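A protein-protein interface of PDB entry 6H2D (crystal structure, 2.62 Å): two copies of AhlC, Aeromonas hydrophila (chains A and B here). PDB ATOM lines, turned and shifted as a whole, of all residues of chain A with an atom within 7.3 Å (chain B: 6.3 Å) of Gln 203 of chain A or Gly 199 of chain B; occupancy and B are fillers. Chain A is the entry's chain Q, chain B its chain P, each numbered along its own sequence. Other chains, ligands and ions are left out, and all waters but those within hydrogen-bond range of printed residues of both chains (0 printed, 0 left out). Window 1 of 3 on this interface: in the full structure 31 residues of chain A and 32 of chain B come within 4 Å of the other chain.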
ATOM      1  N   GLN A  15     -18.998  32.626  28.209  1.00  0.00           N
ATOM      2  CA  GLN A  15     -20.090  31.636  28.389  1.00  0.00           C
ATOM      3  C   GLN A  15     -20.101  30.628  27.226  1.00  0.00           C
ATOM      4  O   GLN A  15     -20.161  29.411  27.440  1.00  0.00           O
ATOM      5  CB  GLN A  15     -21.456  32.317  28.548  1.00  0.00           C
ATOM      6  CG  GLN A  15     -21.687  32.940  29.933  1.00  0.00           C
ATOM      7  CD  GLN A  15     -23.139  33.199  30.290  1.00  0.00           C
ATOM      8  OE1 GLN A  15     -23.838  32.338  30.833  1.00  0.00           O
ATOM      9  NE2 GLN A  15     -23.596  34.410  30.025  1.00  0.00           N
ATOM     10  N   ALA A  16     -20.019  31.137  25.993  1.00  0.00           N
ATOM     11  CA  ALA A  16     -20.035  30.301  24.779  1.00  0.00           C
ATOM     12  C   ALA A  16     -18.922  29.236  24.841  1.00  0.00           C
ATOM     13  O   ALA A  16     -19.105  28.125  24.377  1.00  0.00           O
ATOM     14  CB  ALA A  16     -19.919  31.170  23.537  1.00  0.00           C
ATOM     15  N   GLU A  17     -17.772  29.577  25.421  1.00  0.00           N
ATOM     16  CA  GLU A  17     -16.553  28.761  25.300  1.00  0.00           C
ATOM     17  C   GLU A  17     -16.551  27.596  26.290  1.00  0.00           C
ATOM     18  O   GLU A  17     -15.902  26.623  26.052  1.00  0.00           O
ATOM     19  CB  GLU A  17     -15.297  29.603  25.544  1.00  0.00           C
ATOM     20  CG  GLU A  17     -13.995  28.854  25.305  1.00  0.00           C
ATOM     21  CD  GLU A  17     -13.328  28.259  26.521  1.00  0.00           C
ATOM     22  OE1 GLU A  17     -13.755  28.587  27.638  1.00  0.00           O
ATOM     23  OE2 GLU A  17     -12.374  27.499  26.341  1.00  0.00           O
ATOM     24  N   ALA A  18     -17.226  27.747  27.424  1.00  0.00           N
ATOM     25  CA  ALA A  18     -17.371  26.687  28.418  1.00  0.00           C
ATOM     26  C   ALA A  18     -18.157  25.518  27.796  1.00  0.00           C
ATOM     27  O   ALA A  18     -17.758  24.344  27.894  1.00  0.00           O
ATOM     28  CB  ALA A  18     -18.047  27.260  29.649  1.00  0.00           C
ATOM     29  N   THR A  19     -19.277  25.856  27.139  1.00  0.00           N
ATOM     30  CA  THR A  19     -20.074  24.906  26.355  1.00  0.00           C
ATOM     31  C   THR A  19     -19.220  24.279  25.242  1.00  0.00           C
ATOM     32  O   THR A  19     -19.311  23.081  24.981  1.00  0.00           O
ATOM     33  CB  THR A  19     -21.320  25.578  25.756  1.00  0.00           C
ATOM     34  OG1 THR A  19     -21.926  26.364  26.786  1.00  0.00           O
ATOM     35  CG2 THR A  19     -22.312  24.577  25.206  1.00  0.00           C
ATOM     36  N   ILE A  20     -18.416  25.099  24.559  1.00  0.00           N
ATOM     37  CA  ILE A  20     -17.611  24.606  23.437  1.00  0.00           C
ATOM     38  C   ILE A  20     -16.591  23.557  23.914  1.00  0.00           C
ATOM     39  O   ILE A  20     -16.411  22.579  23.215  1.00  0.00           O
ATOM     40  CB  ILE A  20     -16.951  25.769  22.684  1.00  0.00           C
ATOM     41  CG1 ILE A  20     -17.995  26.526  21.855  1.00  0.00           C
ATOM     42  CG2 ILE A  20     -15.805  25.245  21.831  1.00  0.00           C
ATOM     43  CD1 ILE A  20     -17.567  27.912  21.413  1.00  0.00           C
ATOM     44  N   PHE A  23     -17.896  19.648  24.487  1.00  0.00           N
ATOM     45  CA  PHE A  23     -18.053  18.659  23.411  1.00  0.00           C
ATOM     46  C   PHE A  23     -16.823  17.738  23.409  1.00  0.00           C
ATOM     47  O   PHE A  23     -15.697  18.155  23.716  1.00  0.00           O
ATOM     48  CB  PHE A  23     -18.313  19.320  22.051  1.00  0.00           C
ATOM     49  CG  PHE A  23     -19.673  19.961  21.935  1.00  0.00           C
ATOM     50  CD1 PHE A  23     -19.893  21.264  22.366  1.00  0.00           C
ATOM     51  CD2 PHE A  23     -20.764  19.243  21.461  1.00  0.00           C
ATOM     52  CE1 PHE A  23     -21.159  21.835  22.302  1.00  0.00           C
ATOM     53  CE2 PHE A  23     -22.032  19.813  21.409  1.00  0.00           C
ATOM     54  CZ  PHE A  23     -22.227  21.106  21.826  1.00  0.00           C
ATOM     55  N   ILE A  33     -11.238  24.270  16.641  1.00  0.00           N
ATOM     56  CA  ILE A  33     -12.021  25.387  17.143  1.00  0.00           C
ATOM     57  C   ILE A  33     -11.870  25.413  18.659  1.00  0.00           C
ATOM     58  O   ILE A  33     -11.572  26.445  19.221  1.00  0.00           O
ATOM     59  CB  ILE A  33     -13.501  25.323  16.726  1.00  0.00           C
ATOM     60  CG1 ILE A  33     -13.695  25.709  15.253  1.00  0.00           C
ATOM     61  CG2 ILE A  33     -14.351  26.189  17.652  1.00  0.00           C
ATOM     62  CD1 ILE A  33     -15.062  25.328  14.652  1.00  0.00           C
ATOM     63  N   ASN A 117     -15.428  26.510  10.764  1.00  0.00           N
ATOM     64  CA  ASN A 117     -16.879  26.611  10.647  1.00  0.00           C
ATOM     65  C   ASN A 117     -17.367  25.997   9.331  1.00  0.00           C
ATOM     66  O   ASN A 117     -18.112  25.018   9.335  1.00  0.00           O
ATOM     67  CB  ASN A 117     -17.354  28.053  10.729  1.00  0.00           C
ATOM     68  CG  ASN A 117     -18.468  28.243  11.740  1.00  0.00           C
ATOM     69  OD1 ASN A 117     -19.605  27.811  11.509  1.00  0.00           O
ATOM     70  ND2 ASN A 117     -18.142  28.908  12.844  1.00  0.00           N
ATOM     71  N   GLN A 197     -23.153  17.848  16.182  1.00  0.00           N
ATOM     72  CA  GLN A 197     -22.499  18.818  15.298  1.00  0.00           C
ATOM     73  C   GLN A 197     -23.396  20.032  15.055  1.00  0.00           C
ATOM     74  O   GLN A 197     -22.927  21.152  15.123  1.00  0.00           O
ATOM     75  CB  GLN A 197     -22.087  18.188  13.980  1.00  0.00           C
ATOM     76  CG  GLN A 197     -20.866  17.291  14.105  1.00  0.00           C
ATOM     77  CD  GLN A 197     -20.410  16.833  12.737  1.00  0.00           C
ATOM     78  OE1 GLN A 197     -20.517  17.584  11.757  1.00  0.00           O
ATOM     79  NE2 GLN A 197     -19.930  15.596  12.666  1.00  0.00           N
ATOM     80  N   GLN A 198     -24.670  19.830  14.721  1.00  0.00           N
ATOM     81  CA  GLN A 198     -25.521  20.961  14.680  1.00  0.00           C
ATOM     82  C   GLN A 198     -25.273  21.766  15.964  1.00  0.00           C
ATOM     83  O   GLN A 198     -25.084  22.964  15.908  1.00  0.00           O
ATOM     84  CB  GLN A 198     -26.977  20.534  14.555  1.00  0.00           C
ATOM     85  CG  GLN A 198     -27.427  20.195  13.140  1.00  0.00           C
ATOM     86  CD  GLN A 198     -28.678  19.336  13.117  1.00  0.00           C
ATOM     87  OE1 GLN A 198     -29.415  19.210  14.115  1.00  0.00           O
ATOM     88  NE2 GLN A 198     -28.935  18.739  11.958  1.00  0.00           N
ATOM     89  N   GLY A 199     -25.230  21.082  17.120  1.00  0.00           N
ATOM     90  CA  GLY A 199     -25.070  21.715  18.435  1.00  0.00           C
ATOM     91  C   GLY A 199     -23.816  22.567  18.546  1.00  0.00           C
ATOM     92  O   GLY A 199     -23.837  23.750  18.989  1.00  0.00           O
ATOM     93  N   PHE A 200     -22.698  21.959  18.150  1.00  0.00           N
ATOM     94  CA  PHE A 200     -21.388  22.594  18.191  1.00  0.00           C
ATOM     95  C   PHE A 200     -21.398  23.807  17.273  1.00  0.00           C
ATOM     96  O   PHE A 200     -21.065  24.890  17.695  1.00  0.00           O
ATOM     97  CB  PHE A 200     -20.303  21.602  17.768  1.00  0.00           C
ATOM     98  CG  PHE A 200     -18.906  22.051  18.091  1.00  0.00           C
ATOM     99  CD1 PHE A 200     -18.465  22.070  19.402  1.00  0.00           C
ATOM    100  CD2 PHE A 200     -18.035  22.444  17.095  1.00  0.00           C
ATOM    101  CE1 PHE A 200     -17.174  22.470  19.714  1.00  0.00           C
ATOM    102  CE2 PHE A 200     -16.751  22.865  17.405  1.00  0.00           C
ATOM    103  CZ  PHE A 200     -16.323  22.886  18.715  1.00  0.00           C
ATOM    104  N   LEU A 201     -21.771  23.604  16.009  1.00  0.00           N
ATOM    105  CA  LEU A 201     -21.735  24.685  15.062  1.00  0.00           C
ATOM    106  C   LEU A 201     -22.630  25.807  15.583  1.00  0.00           C
ATOM    107  O   LEU A 201     -22.231  26.966  15.521  1.00  0.00           O
ATOM    108  CB  LEU A 201     -22.158  24.215  13.667  1.00  0.00           C
ATOM    109  CG  LEU A 201     -21.022  23.616  12.841  1.00  0.00           C
ATOM    110  CD1 LEU A 201     -21.543  22.933  11.594  1.00  0.00           C
ATOM    111  CD2 LEU A 201     -19.998  24.677  12.483  1.00  0.00           C
ATOM    112  N   GLY A 202     -23.775  25.442  16.177  1.00  0.00           N
ATOM    113  CA  GLY A 202     -24.618  26.397  16.840  1.00  0.00           C
ATOM    114  C   GLY A 202     -23.811  27.359  17.691  1.00  0.00           C
ATOM    115  O   GLY A 202     -24.047  28.522  17.674  1.00  0.00           O
ATOM    116  N   GLN A 203     -22.834  26.847  18.439  1.00  0.00           N
ATOM    117  CA  GLN A 203     -22.163  27.618  19.447  1.00  0.00           C
ATOM    118  C   GLN A 203     -20.971  28.359  18.841  1.00  0.00           C
ATOM    119  O   GLN A 203     -20.839  29.566  19.048  1.00  0.00           O
ATOM    120  CB  GLN A 203     -21.731  26.725  20.595  1.00  0.00           C
ATOM    121  CG  GLN A 203     -22.897  26.086  21.322  1.00  0.00           C
ATOM    122  CD  GLN A 203     -23.436  26.932  22.441  1.00  0.00           C
ATOM    123  OE1 GLN A 203     -22.721  27.364  23.337  1.00  0.00           O
ATOM    124  NE2 GLN A 203     -24.733  27.138  22.420  1.00  0.00           N
ATOM    125  N   THR A 204     -20.136  27.667  18.069  1.00  0.00           N
ATOM    126  CA  THR A 204     -18.996  28.361  17.455  1.00  0.00           C
ATOM    127  C   THR A 204     -19.516  29.514  16.585  1.00  0.00           C
ATOM    128  O   THR A 204     -18.985  30.565  16.577  1.00  0.00           O
ATOM    129  CB  THR A 204     -18.074  27.425  16.669  1.00  0.00           C
ATOM    130  OG1 THR A 204     -18.783  27.049  15.492  1.00  0.00           O
ATOM    131  CG2 THR A 204     -17.645  26.206  17.458  1.00  0.00           C
ATOM    132  N   THR A 205     -20.624  29.312  15.899  1.00  0.00           N
ATOM    133  CA  THR A 205     -21.232  30.356  15.097  1.00  0.00           C
ATOM    134  C   THR A 205     -21.639  31.550  15.956  1.00  0.00           C
ATOM    135  O   THR A 205     -21.439  32.695  15.533  1.00  0.00           O
ATOM    136  CB  THR A 205     -22.423  29.796  14.328  1.00  0.00           C
ATOM    137  OG1 THR A 205     -21.720  29.100  13.295  1.00  0.00           O
ATOM    138  CG2 THR A 205     -23.372  30.853  13.818  1.00  0.00           C
ATOM    139  N   ALA A 206     -22.198  31.279  17.141  1.00  0.00           N
ATOM    140  CA  ALA A 206     -22.633  32.331  18.048  1.00  0.00           C
ATOM    141  C   ALA A 206     -21.386  33.027  18.617  1.00  0.00           C
ATOM    142  O   ALA A 206     -21.251  34.275  18.559  1.00  0.00           O
ATOM    143  CB  ALA A 206     -23.560  31.771  19.104  1.00  0.00           C
ATOM    144  N   PHE A 207     -20.428  32.218  19.063  1.00  0.00           N
ATOM    145  CA  PHE A 207     -19.106  32.732  19.468  1.00  0.00           C
ATOM    146  C   PHE A 207     -18.526  33.641  18.374  1.00  0.00           C
ATOM    147  O   PHE A 207     -18.056  34.752  18.665  1.00  0.00           O
ATOM    148  CB  PHE A 207     -18.125  31.595  19.772  1.00  0.00           C
ATOM    149  CG  PHE A 207     -16.884  32.060  20.486  1.00  0.00           C
ATOM    150  CD1 PHE A 207     -15.889  32.746  19.808  1.00  0.00           C
ATOM    151  CD2 PHE A 207     -16.719  31.850  21.845  1.00  0.00           C
ATOM    152  CE1 PHE A 207     -14.750  33.167  20.469  1.00  0.00           C
ATOM    153  CE2 PHE A 207     -15.578  32.279  22.505  1.00  0.00           C
ATOM    154  CZ  PHE A 207     -14.601  32.933  21.813  1.00  0.00           C
ATOM    155  N   SER A 208     -18.554  33.160  17.126  1.00  0.00           N
ATOM    156  CA  SER A 208     -17.933  33.848  16.023  1.00  0.00           C
ATOM    157  C   SER A 208     -18.684  35.144  15.695  1.00  0.00           C
ATOM    158  O   SER A 208     -18.076  36.068  15.209  1.00  0.00           O
ATOM    159  CB  SER A 208     -17.819  32.982  14.798  1.00  0.00           C
ATOM    160  OG  SER A 208     -17.101  33.669  13.768  1.00  0.00           O
ATOM    161  N   GLN A 209     -19.993  35.209  15.954  1.00  0.00           N
ATOM    162  CA  GLN A 209     -20.711  36.433  15.665  1.00  0.00           C
ATOM    163  C   GLN A 209     -20.389  37.472  16.761  1.00  0.00           C
ATOM    164  O   GLN A 209     -20.057  38.601  16.453  1.00  0.00           O
ATOM    165  CB  GLN A 209     -22.199  36.137  15.388  1.00  0.00           C
ATOM    166  CG  GLN A 209     -22.525  36.049  13.886  1.00  0.00           C
ATOM    167  CD  GLN A 209     -23.486  34.950  13.469  1.00  0.00           C
ATOM    168  OE1 GLN A 209     -24.402  34.578  14.205  1.00  0.00           O
ATOM    169  NE2 GLN A 209     -23.299  34.419  12.265  1.00  0.00           N
ATOM    170  N   SER B  22     -23.313  22.775  31.084  1.00  0.00           N
ATOM    171  CA  SER B  22     -22.328  23.817  30.833  1.00  0.00           C
ATOM    172  C   SER B  22     -22.957  25.208  30.854  1.00  0.00           C
ATOM    173  O   SER B  22     -22.255  26.156  31.033  1.00  0.00           O
ATOM    174  CB  SER B  22     -21.582  23.574  29.525  1.00  0.00           C
ATOM    175  OG  SER B  22     -22.057  24.410  28.479  1.00  0.00           O
ATOM    176  N   PHE B  23     -24.273  25.302  30.643  1.00  0.00           N
ATOM    177  CA  PHE B  23     -25.007  26.595  30.606  1.00  0.00           C
ATOM    178  C   PHE B  23     -25.280  27.148  32.011  1.00  0.00           C
ATOM    179  O   PHE B  23     -25.614  26.420  32.944  1.00  0.00           O
ATOM    180  CB  PHE B  23     -26.326  26.424  29.855  1.00  0.00           C
ATOM    181  CG  PHE B  23     -26.119  26.114  28.394  1.00  0.00           C
ATOM    182  CD1 PHE B  23     -25.868  24.814  27.968  1.00  0.00           C
ATOM    183  CD2 PHE B  23     -26.121  27.130  27.458  1.00  0.00           C
ATOM    184  CE1 PHE B  23     -25.693  24.527  26.622  1.00  0.00           C
ATOM    185  CE2 PHE B  23     -25.911  26.850  26.119  1.00  0.00           C
ATOM    186  CZ  PHE B  23     -25.708  25.546  25.697  1.00  0.00           C
ATOM    187  N   ILE B 194     -30.841  35.509  23.882  1.00  0.00           N
ATOM    188  CA  ILE B 194     -31.501  34.798  22.779  1.00  0.00           C
ATOM    189  C   ILE B 194     -30.556  33.710  22.238  1.00  0.00           C
ATOM    190  O   ILE B 194     -30.999  32.585  22.029  1.00  0.00           O
ATOM    191  CB  ILE B 194     -31.921  35.787  21.686  1.00  0.00           C
ATOM    192  CG1 ILE B 194     -33.244  36.461  22.039  1.00  0.00           C
ATOM    193  CG2 ILE B 194     -31.956  35.125  20.306  1.00  0.00           C
ATOM    194  CD1 ILE B 194     -33.633  37.573  21.077  1.00  0.00           C
ATOM    195  N   GLN B 195     -29.274  34.061  22.032  1.00  0.00           N
ATOM    196  CA  GLN B 195     -28.237  33.131  21.518  1.00  0.00           C
ATOM    197  C   GLN B 195     -28.095  31.908  22.447  1.00  0.00           C
ATOM    198  O   GLN B 195     -27.986  30.761  21.967  1.00  0.00           O
ATOM    199  CB  GLN B 195     -26.877  33.828  21.360  1.00  0.00           C
ATOM    200  CG  GLN B 195     -26.555  34.276  19.939  1.00  0.00           C
ATOM    201  CD  GLN B 195     -25.387  35.232  19.823  1.00  0.00           C
ATOM    202  OE1 GLN B 195     -24.836  35.721  20.814  1.00  0.00           O
ATOM    203  NE2 GLN B 195     -25.004  35.520  18.590  1.00  0.00           N
ATOM    204  N   ARG B 196     -28.066  32.163  23.759  1.00  0.00           N
ATOM    205  CA  ARG B 196     -27.798  31.132  24.697  1.00  0.00           C
ATOM    206  C   ARG B 196     -28.974  30.157  24.725  1.00  0.00           C
ATOM    207  O   ARG B 196     -28.769  28.957  24.774  1.00  0.00           O
ATOM    208  CB  ARG B 196     -27.494  31.682  26.097  1.00  0.00           C
ATOM    209  CG  ARG B 196     -26.003  31.842  26.370  1.00  0.00           C
ATOM    210  CD  ARG B 196     -25.695  32.301  27.780  1.00  0.00           C
ATOM    211  NE  ARG B 196     -26.492  33.442  28.219  1.00  0.00           N
ATOM    212  CZ  ARG B 196     -26.169  34.723  28.033  1.00  0.00           C
ATOM    213  NH1 ARG B 196     -25.038  35.048  27.427  1.00  0.00           N
ATOM    214  NH2 ARG B 196     -26.982  35.678  28.454  1.00  0.00           N
ATOM    215  N   GLN B 197     -30.193  30.701  24.734  1.00  0.00           N
ATOM    216  CA  GLN B 197     -31.372  29.938  25.026  1.00  0.00           C
ATOM    217  C   GLN B 197     -31.721  29.047  23.817  1.00  0.00           C
ATOM    218  O   GLN B 197     -32.292  27.954  23.992  1.00  0.00           O
ATOM    219  CB  GLN B 197     -32.513  30.892  25.398  1.00  0.00           C
ATOM    220  CG  GLN B 197     -32.549  31.306  26.865  1.00  0.00           C
ATOM    221  CD  GLN B 197     -33.753  32.162  27.196  1.00  0.00           C
ATOM    222  OE1 GLN B 197     -34.729  32.235  26.441  1.00  0.00           O
ATOM    223  NE2 GLN B 197     -33.701  32.822  28.344  1.00  0.00           N
ATOM    224  N   GLN B 198     -31.398  29.539  22.604  1.00  0.00           N
ATOM    225  CA  GLN B 198     -31.493  28.796  21.339  1.00  0.00           C
ATOM    226  C   GLN B 198     -30.538  27.603  21.344  1.00  0.00           C
ATOM    227  O   GLN B 198     -30.942  26.520  20.975  1.00  0.00           O
ATOM    228  CB  GLN B 198     -31.126  29.650  20.132  1.00  0.00           C
ATOM    229  CG  GLN B 198     -32.285  30.451  19.583  1.00  0.00           C
ATOM    230  CD  GLN B 198     -31.848  31.651  18.771  1.00  0.00           C
ATOM    231  OE1 GLN B 198     -30.680  32.091  18.790  1.00  0.00           O
ATOM    232  NE2 GLN B 198     -32.824  32.206  18.062  1.00  0.00           N
ATOM    233  N   GLY B 199     -29.286  27.836  21.752  1.00  0.00           N
ATOM    234  CA  GLY B 199     -28.266  26.778  21.919  1.00  0.00           C
ATOM    235  C   GLY B 199     -28.742  25.666  22.843  1.00  0.00           C
ATOM    236  O   GLY B 199     -28.916  24.486  22.406  1.00  0.00           O
ATOM    237  N   PHE B 200     -28.993  26.066  24.103  1.00  0.00           N
ATOM    238  CA  PHE B 200     -29.537  25.233  25.139  1.00  0.00           C
ATOM    239  C   PHE B 200     -30.670  24.370  24.573  1.00  0.00           C
ATOM    240  O   PHE B 200     -30.605  23.159  24.555  1.00  0.00           O
ATOM    241  CB  PHE B 200     -30.001  26.072  26.319  1.00  0.00           C
ATOM    242  CG  PHE B 200     -30.332  25.240  27.533  1.00  0.00           C
ATOM    243  CD1 PHE B 200     -29.326  24.701  28.323  1.00  0.00           C
ATOM    244  CD2 PHE B 200     -31.642  24.975  27.882  1.00  0.00           C
ATOM    245  CE1 PHE B 200     -29.624  23.915  29.424  1.00  0.00           C
ATOM    246  CE2 PHE B 200     -31.935  24.195  28.992  1.00  0.00           C
ATOM    247  CZ  PHE B 200     -30.933  23.664  29.762  1.00  0.00           C
ATOM    248  N   LEU B 201     -31.682  25.019  24.037  1.00  0.00           N
ATOM    249  CA  LEU B 201     -32.872  24.357  23.508  1.00  0.00           C
ATOM    250  C   LEU B 201     -32.497  23.325  22.432  1.00  0.00           C
ATOM    251  O   LEU B 201     -33.087  22.247  22.370  1.00  0.00           O
ATOM    252  CB  LEU B 201     -33.753  25.473  22.934  1.00  0.00           C
ATOM    253  CG  LEU B 201     -35.204  25.148  22.649  1.00  0.00           C
ATOM    254  CD1 LEU B 201     -35.728  24.117  23.651  1.00  0.00           C
ATOM    255  CD2 LEU B 201     -36.006  26.450  22.668  1.00  0.00           C
ATOM    256  N   GLY B 202     -31.511  23.636  21.576  1.00  0.00           N
ATOM    257  CA  GLY B 202     -30.999  22.650  20.584  1.00  0.00           C
ATOM    258  C   GLY B 202     -30.578  21.336  21.266  1.00  0.00           C
ATOM    259  O   GLY B 202     -30.779  20.214  20.751  1.00  0.00           O
ATOM    260  N   GLN B 203     -30.012  21.483  22.468  1.00  0.00           N
ATOM    261  CA  GLN B 203     -29.441  20.420  23.245  1.00  0.00           C
ATOM    262  C   GLN B 203     -30.538  19.536  23.835  1.00  0.00           C
ATOM    263  O   GLN B 203     -30.524  18.345  23.609  1.00  0.00           O
ATOM    264  CB  GLN B 203     -28.578  21.034  24.355  1.00  0.00           C
ATOM    265  CG  GLN B 203     -27.328  21.777  23.869  1.00  0.00           C
ATOM    266  CD  GLN B 203     -26.386  20.864  23.110  1.00  0.00           C
ATOM    267  OE1 GLN B 203     -25.913  21.218  22.040  1.00  0.00           O
ATOM    268  NE2 GLN B 203     -26.123  19.677  23.643  1.00  0.00           N
ATOM    269  N   THR B 204     -31.480  20.146  24.571  1.00  0.00           N
ATOM    270  CA  THR B 204     -32.514  19.435  25.272  1.00  0.00           C
ATOM    271  C   THR B 204     -33.540  18.864  24.290  1.00  0.00           C
ATOM    272  O   THR B 204     -34.042  17.787  24.529  1.00  0.00           O
ATOM    273  CB  THR B 204     -33.205  20.299  26.318  1.00  0.00           C
ATOM    274  OG1 THR B 204     -33.937  21.295  25.613  1.00  0.00           O
ATOM    275  CG2 THR B 204     -32.221  20.910  27.296  1.00  0.00           C
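Hydrophobic or aromatic side chains of chain A within 4 Å of the printed part of chain B: Phe 23 and Ala 206.
Of the 13 printed residues of chain B, 6 touch a printed residue of chain A.
Among the printed residues, no Asp or Glu carboxylate lies within 4 Å of a Lys or Arg side-chain nitrogen of the other chain.
Phe 23 of chain A touches Gln 203 of chain B, and with the chains exchanged Gln 203 of chain A touches Phe 23 of chain B.
Gly 199 of chain A touches Gln 203 of chain B, and with the chains exchanged Gln 203 of chain A touches Gly 199 of chain B.
Of the 8 pairs that touch across the chains among the printed residues, 4 have their exchanged pair printed and touching as well.
The side-chain hydroxyl (OG1) of Thr 19 of chain A sits at hydrogen-bond distance from the side-chain hydroxyl (OG) of Ser 22 of chain B (2.6 Å).
NE2 of Gln 15 of chain A sits close to NH1 of Arg 196 of chain B (3.0 Å).
Among the printed residues, pairs that only touch across the chains: Thr 19 of chain A with Phe 23 of chain B (3.6 Å), Phe 23 of chain A with Gln 203 of chain B (3.7 Å), Gly 199 of chain A with Gln 203 of chain B (3.7 Å), Gln 203 of chain A with Phe 23 of chain B (3.8 Å), Gln 203 of chain A with Gly 199 of chain B (3.6 Å) and Ala 206 of chain A with Gln 195 of chain B (3.95 Å).
Printed residues of chain B within 4 Å of Gln 15 of chain A: Arg 196.
Printed residues of chain B within 4 Å of Thr 19 of chain A: Ser 22 and Phe 23.
Printed residues of chain B within 4 Å of Phe 23 of chain A: Gln 203.
Printed residues of chain B within 4 Å of Gly 199 of chain A: Gln 203 (3.7 Å).
Gln 203 of chain A touches two residues of chain B.
Thr 205 of chain A touches none of the printed residues of chain B.
Of the printed residues of chain A, Phe 23 of chain B touches Thr 19 and Gln 203.
Gly 199 of chain B touches just one residue of chain A: Gln 203 (3.6 Å).
The nearest printed residue of chain B that does not touch Gln 15 of chain A is Ser 22 of chain B (5.3 Å).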
